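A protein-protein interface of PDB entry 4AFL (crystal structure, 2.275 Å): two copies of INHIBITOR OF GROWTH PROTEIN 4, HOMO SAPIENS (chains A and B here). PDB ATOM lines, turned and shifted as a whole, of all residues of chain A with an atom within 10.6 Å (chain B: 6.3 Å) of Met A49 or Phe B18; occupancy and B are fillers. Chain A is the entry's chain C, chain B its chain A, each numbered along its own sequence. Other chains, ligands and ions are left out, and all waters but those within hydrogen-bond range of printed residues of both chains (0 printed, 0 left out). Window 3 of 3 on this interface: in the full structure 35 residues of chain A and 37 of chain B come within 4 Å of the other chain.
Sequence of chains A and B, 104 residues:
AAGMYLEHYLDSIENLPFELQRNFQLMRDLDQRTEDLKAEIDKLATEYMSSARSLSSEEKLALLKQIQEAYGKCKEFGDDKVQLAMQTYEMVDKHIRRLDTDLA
No position is printed for both chains.
Of the 5 pairs that touch across the chains among the printed residues, none has its exchanged pair printed and touching as well.
Hydrophobic or aromatic side chains of chain B within 4 Å of the printed part of chain A: Leu B16, Pro B17 and Phe B18.
Along chain A the printed residues that touch a printed residue of chain B span positions 48 to 64.
Among the printed residues, 5 pairs touch across the chains.
Pro B17 touches Tyr A48 (CD to CE2, 3.3 Å).
Met A49 touches Pro B17.
Met A49 touches Phe B18.
Met A49 touches Gln B21.
CD2 of Leu A64 touches CD2 of Leu B16, 3.6 Å away.
Of the printed residues of chain B, Tyr A48 touches Pro B17.
Of chain B, only Pro B17 (3.6 Å), Phe B18 (3.96 Å) and Gln B21 (3.2 Å) come within 4 Å of Met A49.
Of the printed residues of chain B, Leu A64 touches Leu B16.
Of the printed residues of chain A, Leu B16 touches Leu A64.
Pro B17 touches two residues of chain A.
Phe B18 touches just one residue of chain A: Met A49.
No residue of chain A comes within 4 Å of Glu B19.
Gln B21 touches just one residue of chain A: Met A49.
The nearest printed residue of chain B that does not touch Tyr A48 is Leu B16 (4.3 Å).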
ATOM      1  N   ILE A  41      21.555  -7.262  -7.018  1.00  0.00           N
ATOM      2  CA  ILE A  41      22.112  -5.922  -7.049  1.00  0.00           C
ATOM      3  C   ILE A  41      21.174  -4.954  -7.770  1.00  0.00           C
ATOM      4  O   ILE A  41      21.008  -3.809  -7.344  1.00  0.00           O
ATOM      5  CB  ILE A  41      23.457  -5.936  -7.745  1.00  0.00           C
ATOM      6  CG1 ILE A  41      24.480  -6.665  -6.867  1.00  0.00           C
ATOM      7  CG2 ILE A  41      23.894  -4.525  -8.100  1.00  0.00           C
ATOM      8  CD1 ILE A  41      25.820  -6.899  -7.544  1.00  0.00           C
ATOM      9  N   ASP A  42      20.551  -5.423  -8.846  1.00  0.00           N
ATOM     10  CA  ASP A  42      19.664  -4.586  -9.633  1.00  0.00           C
ATOM     11  C   ASP A  42      18.422  -4.242  -8.813  1.00  0.00           C
ATOM     12  O   ASP A  42      17.944  -3.114  -8.820  1.00  0.00           O
ATOM     13  CB  ASP A  42      19.274  -5.299 -10.926  1.00  0.00           C
ATOM     14  CG  ASP A  42      18.521  -4.399 -11.892  1.00  0.00           C
ATOM     15  OD1 ASP A  42      18.491  -3.166 -11.675  1.00  0.00           O
ATOM     16  OD2 ASP A  42      17.970  -4.925 -12.884  1.00  0.00           O
ATOM     17  N   LYS A  43      17.911  -5.230  -8.098  1.00  0.00           N
ATOM     18  CA  LYS A  43      16.767  -5.023  -7.227  1.00  0.00           C
ATOM     19  C   LYS A  43      17.086  -4.025  -6.097  1.00  0.00           C
ATOM     20  O   LYS A  43      16.271  -3.165  -5.789  1.00  0.00           O
ATOM     21  CB  LYS A  43      16.294  -6.373  -6.680  1.00  0.00           C
ATOM     22  CG  LYS A  43      15.216  -6.309  -5.619  1.00  0.00           C
ATOM     23  CD  LYS A  43      15.018  -7.686  -4.994  1.00  0.00           C
ATOM     24  CE  LYS A  43      14.159  -7.618  -3.736  1.00  0.00           C
ATOM     25  NZ  LYS A  43      12.715  -7.373  -4.042  1.00  0.00           N
ATOM     26  N   LEU A  44      18.272  -4.130  -5.503  1.00  0.00           N
ATOM     27  CA  LEU A  44      18.683  -3.236  -4.413  1.00  0.00           C
ATOM     28  C   LEU A  44      18.940  -1.827  -4.907  1.00  0.00           C
ATOM     29  O   LEU A  44      18.585  -0.859  -4.245  1.00  0.00           O
ATOM     30  CB  LEU A  44      19.953  -3.743  -3.733  1.00  0.00           C
ATOM     31  CG  LEU A  44      19.871  -5.020  -2.896  1.00  0.00           C
ATOM     32  CD1 LEU A  44      21.263  -5.592  -2.619  1.00  0.00           C
ATOM     33  CD2 LEU A  44      19.092  -4.775  -1.585  1.00  0.00           C
ATOM     34  N   ALA A  45      19.576  -1.720  -6.067  1.00  0.00           N
ATOM     35  CA  ALA A  45      19.886  -0.436  -6.655  1.00  0.00           C
ATOM     36  C   ALA A  45      18.599   0.265  -7.067  1.00  0.00           C
ATOM     37  O   ALA A  45      18.438   1.477  -6.872  1.00  0.00           O
ATOM     38  CB  ALA A  45      20.800  -0.618  -7.851  1.00  0.00           C
ATOM     39  N   THR A  46      17.683  -0.507  -7.634  1.00  0.00           N
ATOM     40  CA  THR A  46      16.385   0.009  -8.023  1.00  0.00           C
ATOM     41  C   THR A  46      15.674   0.553  -6.794  1.00  0.00           C
ATOM     42  O   THR A  46      15.059   1.618  -6.833  1.00  0.00           O
ATOM     43  CB  THR A  46      15.556  -1.076  -8.714  1.00  0.00           C
ATOM     44  OG1 THR A  46      16.185  -1.398  -9.964  1.00  0.00           O
ATOM     45  CG2 THR A  46      14.135  -0.584  -8.976  1.00  0.00           C
ATOM     46  N   GLU A  47      15.812  -0.176  -5.695  1.00  0.00           N
ATOM     47  CA  GLU A  47      15.251   0.206  -4.414  1.00  0.00           C
ATOM     48  C   GLU A  47      15.889   1.509  -3.965  1.00  0.00           C
ATOM     49  O   GLU A  47      15.206   2.490  -3.698  1.00  0.00           O
ATOM     50  CB  GLU A  47      15.579  -0.883  -3.409  1.00  0.00           C
ATOM     51  CG  GLU A  47      14.526  -1.178  -2.378  1.00  0.00           C
ATOM     52  CD  GLU A  47      14.668  -2.601  -1.854  1.00  0.00           C
ATOM     53  OE1 GLU A  47      14.206  -3.542  -2.549  1.00  0.00           O
ATOM     54  OE2 GLU A  47      15.262  -2.780  -0.763  1.00  0.00           O
ATOM     55  N   TYR A  48      17.216   1.508  -3.893  1.00  0.00           N
ATOM     56  CA  TYR A  48      17.970   2.672  -3.459  1.00  0.00           C
ATOM     57  C   TYR A  48      17.640   3.911  -4.285  1.00  0.00           C
ATOM     58  O   TYR A  48      17.414   4.985  -3.746  1.00  0.00           O
ATOM     59  CB  TYR A  48      19.466   2.388  -3.545  1.00  0.00           C
ATOM     60  CG  TYR A  48      20.305   3.532  -3.060  1.00  0.00           C
ATOM     61  CD1 TYR A  48      20.470   3.776  -1.704  1.00  0.00           C
ATOM     62  CD2 TYR A  48      20.926   4.379  -3.955  1.00  0.00           C
ATOM     63  CE1 TYR A  48      21.242   4.841  -1.262  1.00  0.00           C
ATOM     64  CE2 TYR A  48      21.692   5.432  -3.522  1.00  0.00           C
ATOM     65  CZ  TYR A  48      21.848   5.663  -2.182  1.00  0.00           C
ATOM     66  OH  TYR A  48      22.617   6.729  -1.781  1.00  0.00           O
ATOM     67  N   MET A  49      17.614   3.748  -5.600  1.00  0.00           N
ATOM     68  CA  MET A  49      17.369   4.849  -6.515  1.00  0.00           C
ATOM     69  C   MET A  49      15.994   5.461  -6.278  1.00  0.00           C
ATOM     70  O   MET A  49      15.821   6.684  -6.367  1.00  0.00           O
ATOM     71  CB  MET A  49      17.499   4.356  -7.962  1.00  0.00           C
ATOM     72  CG  MET A  49      17.153   5.385  -9.028  1.00  0.00           C
ATOM     73  SD  MET A  49      18.400   6.891  -9.166  1.00  0.00           S
ATOM     74  CE  MET A  49      19.495   6.263 -10.647  1.00  0.00           C
ATOM     75  N   SER A  50      15.022   4.620  -5.940  1.00  0.00           N
ATOM     76  CA  SER A  50      13.651   5.092  -5.832  1.00  0.00           C
ATOM     77  C   SER A  50      13.290   5.646  -4.447  1.00  0.00           C
ATOM     78  O   SER A  50      12.168   6.115  -4.232  1.00  0.00           O
ATOM     79  CB  SER A  50      12.669   3.994  -6.263  1.00  0.00           C
ATOM     80  OG  SER A  50      12.637   2.932  -5.330  1.00  0.00           O
ATOM     81  N   SER A  51      14.230   5.615  -3.511  1.00  0.00           N
ATOM     82  CA  SER A  51      13.909   6.038  -2.152  1.00  0.00           C
ATOM     83  C   SER A  51      15.008   6.859  -1.475  1.00  0.00           C
ATOM     84  O   SER A  51      14.817   7.352  -0.362  1.00  0.00           O
ATOM     85  CB  SER A  51      13.579   4.822  -1.287  1.00  0.00           C
ATOM     86  OG  SER A  51      14.750   4.069  -1.035  1.00  0.00           O
ATOM     87  N   ALA A  52      16.138   7.028  -2.152  1.00  0.00           N
ATOM     88  CA  ALA A  52      17.332   7.603  -1.521  1.00  0.00           C
ATOM     89  C   ALA A  52      17.198   9.044  -1.008  1.00  0.00           C
ATOM     90  O   ALA A  52      18.058   9.532  -0.269  1.00  0.00           O
ATOM     91  CB  ALA A  52      18.505   7.508  -2.452  1.00  0.00           C
ATOM     92  N   ARG A  53      16.146   9.741  -1.411  1.00  0.00           N
ATOM     93  CA  ARG A  53      15.979  11.124  -0.975  1.00  0.00           C
ATOM     94  C   ARG A  53      15.403  11.207   0.450  1.00  0.00           C
ATOM     95  O   ARG A  53      15.615  12.183   1.158  1.00  0.00           O
ATOM     96  CB  ARG A  53      15.105  11.903  -1.961  1.00  0.00           C
ATOM     97  CG  ARG A  53      15.560  13.331  -2.187  1.00  0.00           C
ATOM     98  CD  ARG A  53      14.479  14.165  -2.900  1.00  0.00           C
ATOM     99  NE  ARG A  53      14.217  13.698  -4.259  1.00  0.00           N
ATOM    100  CZ  ARG A  53      13.391  14.294  -5.111  1.00  0.00           C
ATOM    101  NH1 ARG A  53      12.739  15.389  -4.749  1.00  0.00           N
ATOM    102  NH2 ARG A  53      13.211  13.795  -6.332  1.00  0.00           N
ATOM    103  N   SER A  54      14.684  10.176   0.870  1.00  0.00           N
ATOM    104  CA  SER A  54      13.994  10.208   2.160  1.00  0.00           C
ATOM    105  C   SER A  54      14.592   9.187   3.141  1.00  0.00           C
ATOM    106  O   SER A  54      13.975   8.832   4.153  1.00  0.00           O
ATOM    107  CB  SER A  54      12.514   9.890   1.952  1.00  0.00           C
ATOM    108  OG  SER A  54      12.340   8.491   1.732  1.00  0.00           O
ATOM    109  N   LEU A  55      15.789   8.710   2.827  1.00  0.00           N
ATOM    110  CA  LEU A  55      16.395   7.614   3.569  1.00  0.00           C
ATOM    111  C   LEU A  55      17.224   8.145   4.727  1.00  0.00           C
ATOM    112  O   LEU A  55      17.960   9.119   4.576  1.00  0.00           O
ATOM    113  CB  LEU A  55      17.274   6.787   2.635  1.00  0.00           C
ATOM    114  CG  LEU A  55      16.982   5.294   2.477  1.00  0.00           C
ATOM    115  CD1 LEU A  55      15.489   5.006   2.440  1.00  0.00           C
ATOM    116  CD2 LEU A  55      17.645   4.778   1.216  1.00  0.00           C
ATOM    117  N   GLU A  59      19.136   3.446   7.319  1.00  0.00           N
ATOM    118  CA  GLU A  59      18.510   2.796   6.180  1.00  0.00           C
ATOM    119  C   GLU A  59      19.444   2.817   4.969  1.00  0.00           C
ATOM    120  O   GLU A  59      19.563   1.830   4.239  1.00  0.00           O
ATOM    121  CB  GLU A  59      17.187   3.481   5.818  1.00  0.00           C
ATOM    122  CG  GLU A  59      16.102   3.454   6.909  1.00  0.00           C
ATOM    123  CD  GLU A  59      14.869   4.310   6.548  1.00  0.00           C
ATOM    124  OE1 GLU A  59      14.999   5.542   6.347  1.00  0.00           O
ATOM    125  OE2 GLU A  59      13.759   3.746   6.466  1.00  0.00           O
ATOM    126  N   LYS A  60      20.105   3.946   4.747  1.00  0.00           N
ATOM    127  CA  LYS A  60      20.998   4.036   3.613  1.00  0.00           C
ATOM    128  C   LYS A  60      22.155   3.059   3.835  1.00  0.00           C
ATOM    129  O   LYS A  60      22.602   2.393   2.903  1.00  0.00           O
ATOM    130  CB  LYS A  60      21.482   5.458   3.419  1.00  0.00           C
ATOM    131  CG  LYS A  60      21.966   5.764   2.028  1.00  0.00           C
ATOM    132  CD  LYS A  60      22.232   7.262   1.854  1.00  0.00           C
ATOM    133  CE  LYS A  60      20.958   8.051   1.662  1.00  0.00           C
ATOM    134  NZ  LYS A  60      21.278   9.457   1.267  1.00  0.00           N
ATOM    135  N   LEU A  63      21.342  -0.709   3.215  1.00  0.00           N
ATOM    136  CA  LEU A  63      21.097  -0.986   1.808  1.00  0.00           C
ATOM    137  C   LEU A  63      22.408  -0.950   1.028  1.00  0.00           C
ATOM    138  O   LEU A  63      22.677  -1.821   0.205  1.00  0.00           O
ATOM    139  CB  LEU A  63      20.126   0.063   1.278  1.00  0.00           C
ATOM    140  CG  LEU A  63      19.319  -0.076   0.008  1.00  0.00           C
ATOM    141  CD1 LEU A  63      18.749  -1.461  -0.082  1.00  0.00           C
ATOM    142  CD2 LEU A  63      18.196   0.954   0.058  1.00  0.00           C
ATOM    143  N   LEU A  64      23.232   0.057   1.290  1.00  0.00           N
ATOM    144  CA  LEU A  64      24.539   0.107   0.653  1.00  0.00           C
ATOM    145  C   LEU A  64      25.410  -1.097   1.067  1.00  0.00           C
ATOM    146  O   LEU A  64      26.124  -1.673   0.233  1.00  0.00           O
ATOM    147  CB  LEU A  64      25.240   1.420   0.956  1.00  0.00           C
ATOM    148  CG  LEU A  64      24.586   2.712   0.447  1.00  0.00           C
ATOM    149  CD1 LEU A  64      25.494   3.879   0.753  1.00  0.00           C
ATOM    150  CD2 LEU A  64      24.308   2.658  -1.034  1.00  0.00           C
ATOM    151  N   ILE A  67      24.521  -3.959  -1.154  1.00  0.00           N
ATOM    152  CA  ILE A  67      25.030  -3.754  -2.501  1.00  0.00           C
ATOM    153  C   ILE A  67      26.525  -4.039  -2.505  1.00  0.00           C
ATOM    154  O   ILE A  67      27.038  -4.725  -3.384  1.00  0.00           O
ATOM    155  CB  ILE A  67      24.752  -2.318  -2.991  1.00  0.00           C
ATOM    156  CG1 ILE A  67      23.257  -2.123  -3.237  1.00  0.00           C
ATOM    157  CG2 ILE A  67      25.508  -2.022  -4.266  1.00  0.00           C
ATOM    158  CD1 ILE A  67      22.895  -0.687  -3.583  1.00  0.00           C
ATOM    159  N   TYR A  71      28.413  -7.026  -4.414  1.00  0.00           N
ATOM    160  CA  TYR A  71      29.471  -6.750  -5.371  1.00  0.00           C
ATOM    161  C   TYR A  71      30.780  -7.440  -4.994  1.00  0.00           C
ATOM    162  O   TYR A  71      31.495  -7.943  -5.854  1.00  0.00           O
ATOM    163  CB  TYR A  71      29.664  -5.255  -5.544  1.00  0.00           C
ATOM    164  CG  TYR A  71      28.922  -4.703  -6.732  1.00  0.00           C
ATOM    165  CD1 TYR A  71      29.328  -5.009  -8.033  1.00  0.00           C
ATOM    166  CD2 TYR A  71      27.829  -3.869  -6.566  1.00  0.00           C
ATOM    167  CE1 TYR A  71      28.655  -4.497  -9.130  1.00  0.00           C
ATOM    168  CE2 TYR A  71      27.152  -3.349  -7.660  1.00  0.00           C
ATOM    169  CZ  TYR A  71      27.569  -3.666  -8.935  1.00  0.00           C
ATOM    170  OH  TYR A  71      26.891  -3.152 -10.022  1.00  0.00           O
ATOM    171  N   GLU B  14      24.630  11.788  -3.401  1.00  0.00           N
ATOM    172  CA  GLU B  14      23.513  12.016  -4.309  1.00  0.00           C
ATOM    173  C   GLU B  14      23.817  11.434  -5.675  1.00  0.00           C
ATOM    174  O   GLU B  14      22.927  10.906  -6.344  1.00  0.00           O
ATOM    175  CB  GLU B  14      23.166  13.507  -4.427  1.00  0.00           C
ATOM    176  CG  GLU B  14      22.591  14.120  -3.137  1.00  0.00           C
ATOM    177  CD  GLU B  14      23.677  14.577  -2.169  1.00  0.00           C
ATOM    178  OE1 GLU B  14      24.876  14.290  -2.422  1.00  0.00           O
ATOM    179  OE2 GLU B  14      23.334  15.226  -1.157  1.00  0.00           O
ATOM    180  N   ASN B  15      25.081  11.492  -6.084  1.00  0.00           N
ATOM    181  CA  ASN B  15      25.439  10.930  -7.388  1.00  0.00           C
ATOM    182  C   ASN B  15      25.640   9.410  -7.412  1.00  0.00           C
ATOM    183  O   ASN B  15      25.728   8.813  -8.485  1.00  0.00           O
ATOM    184  CB  ASN B  15      26.648  11.654  -7.986  1.00  0.00           C
ATOM    185  CG  ASN B  15      26.332  13.091  -8.342  1.00  0.00           C
ATOM    186  OD1 ASN B  15      25.199  13.405  -8.703  1.00  0.00           O
ATOM    187  ND2 ASN B  15      27.329  13.977  -8.228  1.00  0.00           N
ATOM    188  N   LEU B  16      25.688   8.780  -6.244  1.00  0.00           N
ATOM    189  CA  LEU B  16      25.968   7.342  -6.192  1.00  0.00           C
ATOM    190  C   LEU B  16      25.012   6.475  -7.031  1.00  0.00           C
ATOM    191  O   LEU B  16      25.476   5.711  -7.876  1.00  0.00           O
ATOM    192  CB  LEU B  16      26.038   6.828  -4.762  1.00  0.00           C
ATOM    193  CG  LEU B  16      26.377   5.342  -4.684  1.00  0.00           C
ATOM    194  CD1 LEU B  16      27.833   5.178  -5.049  1.00  0.00           C
ATOM    195  CD2 LEU B  16      26.115   4.780  -3.307  1.00  0.00           C
ATOM    196  N   PRO B  17      23.681   6.594  -6.817  1.00  0.00           N
ATOM    197  CA  PRO B  17      22.809   5.710  -7.608  1.00  0.00           C
ATOM    198  C   PRO B  17      22.961   5.903  -9.107  1.00  0.00           C
ATOM    199  O   PRO B  17      22.779   4.940  -9.839  1.00  0.00           O
ATOM    200  CB  PRO B  17      21.392   6.101  -7.167  1.00  0.00           C
ATOM    201  CG  PRO B  17      21.546   7.415  -6.437  1.00  0.00           C
ATOM    202  CD  PRO B  17      22.914   7.408  -5.853  1.00  0.00           C
ATOM    203  N   PHE B  18      23.311   7.110  -9.543  1.00  0.00           N
ATOM    204  CA  PHE B  18      23.491   7.380 -10.969  1.00  0.00           C
ATOM    205  C   PHE B  18      24.746   6.721 -11.497  1.00  0.00           C
ATOM    206  O   PHE B  18      24.737   6.159 -12.592  1.00  0.00           O
ATOM    207  CB  PHE B  18      23.530   8.887 -11.240  1.00  0.00           C
ATOM    208  CG  PHE B  18      22.265   9.579 -10.864  1.00  0.00           C
ATOM    209  CD1 PHE B  18      21.217   9.654 -11.761  1.00  0.00           C
ATOM    210  CD2 PHE B  18      22.091  10.091  -9.585  1.00  0.00           C
ATOM    211  CE1 PHE B  18      20.018  10.260 -11.403  1.00  0.00           C
ATOM    212  CE2 PHE B  18      20.907  10.706  -9.226  1.00  0.00           C
ATOM    213  CZ  PHE B  18      19.863  10.789 -10.140  1.00  0.00           C
ATOM    214  N   GLU B  19      25.824   6.770 -10.715  1.00  0.00           N
ATOM    215  CA  GLU B  19      27.063   6.180 -11.171  1.00  0.00           C
ATOM    216  C   GLU B  19      26.932   4.662 -11.125  1.00  0.00           C
ATOM    217  O   GLU B  19      27.416   3.968 -12.014  1.00  0.00           O
ATOM    218  CB  GLU B  19      28.258   6.666 -10.344  1.00  0.00           C
ATOM    219  CG  GLU B  19      29.646   6.230 -10.875  1.00  0.00           C
ATOM    220  CD  GLU B  19      30.060   6.892 -12.195  1.00  0.00           C
ATOM    221  OE1 GLU B  19      29.294   7.723 -12.733  1.00  0.00           O
ATOM    222  OE2 GLU B  19      31.171   6.586 -12.687  1.00  0.00           O
ATOM    223  N   LEU B  20      26.265   4.154 -10.098  1.00  0.00           N
ATOM    224  CA  LEU B  20      25.992   2.726 -10.000  1.00  0.00           C
ATOM    225  C   LEU B  20      25.302   2.202 -11.246  1.00  0.00           C
ATOM    226  O   LEU B  20      25.754   1.228 -11.850  1.00  0.00           O
ATOM    227  CB  LEU B  20      25.114   2.421  -8.796  1.00  0.00           C
ATOM    228  CG  LEU B  20      25.877   2.412  -7.488  1.00  0.00           C
ATOM    229  CD1 LEU B  20      25.023   1.772  -6.412  1.00  0.00           C
ATOM    230  CD2 LEU B  20      27.180   1.662  -7.686  1.00  0.00           C
ATOM    231  N   GLN B  21      24.212   2.859 -11.627  1.00  0.00           N
ATOM    232  CA  GLN B  21      23.457   2.464 -12.804  1.00  0.00           C
ATOM    233  C   GLN B  21      24.375   2.456 -14.026  1.00  0.00           C
ATOM    234  O   GLN B  21      24.277   1.582 -14.880  1.00  0.00           O
ATOM    235  CB  GLN B  21      22.302   3.436 -13.026  1.00  0.00           C
ATOM    236  CG  GLN B  21      20.936   2.805 -13.115  1.00  0.00           C
ATOM    237  CD  GLN B  21      19.850   3.845 -13.381  1.00  0.00           C
ATOM    238  OE1 GLN B  21      20.136   5.038 -13.537  1.00  0.00           O
ATOM    239  NE2 GLN B  21      18.600   3.397 -13.437  1.00  0.00           N
ATOM    240  N   ARG B  22      25.267   3.437 -14.093  1.00  0.00           N
ATOM    241  CA  ARG B  22      26.229   3.529 -15.176  1.00  0.00           C
ATOM    242  C   ARG B  22      27.069   2.268 -15.206  1.00  0.00           C
ATOM    243  O   ARG B  22      27.208   1.632 -16.241  1.00  0.00           O
ATOM    244  CB  ARG B  22      27.144   4.734 -14.963  1.00  0.00           C
ATOM    245  CG  ARG B  22      27.634   5.393 -16.233  1.00  0.00           C
ATOM    246  CD  ARG B  22      28.282   6.742 -15.928  1.00  0.00           C
ATOM    247  NE  ARG B  22      28.521   7.507 -17.145  1.00  0.00           N
ATOM    248  CZ  ARG B  22      29.572   7.340 -17.944  1.00  0.00           C
ATOM    249  NH1 ARG B  22      30.503   6.433 -17.656  1.00  0.00           N
ATOM    250  NH2 ARG B  22      29.695   8.093 -19.029  1.00  0.00           N
ATOM    251  N   ASN B  23      27.632   1.912 -14.058  1.00  0.00           N
ATOM    252  CA  ASN B  23      28.472   0.729 -13.953  1.00  0.00           C
ATOM    253  C   ASN B  23      27.719  -0.570 -14.186  1.00  0.00           C
ATOM    254  O   ASN B  23      28.271  -1.528 -14.721  1.00  0.00           O
ATOM    255  CB  ASN B  23      29.147   0.680 -12.600  1.00  0.00           C
ATOM    256  CG  ASN B  23      30.307   1.626 -12.513  1.00  0.00           C
ATOM    257  OD1 ASN B  23      30.519   2.444 -13.412  1.00  0.00           O
ATOM    258  ND2 ASN B  23      31.073   1.527 -11.432  1.00  0.00           N
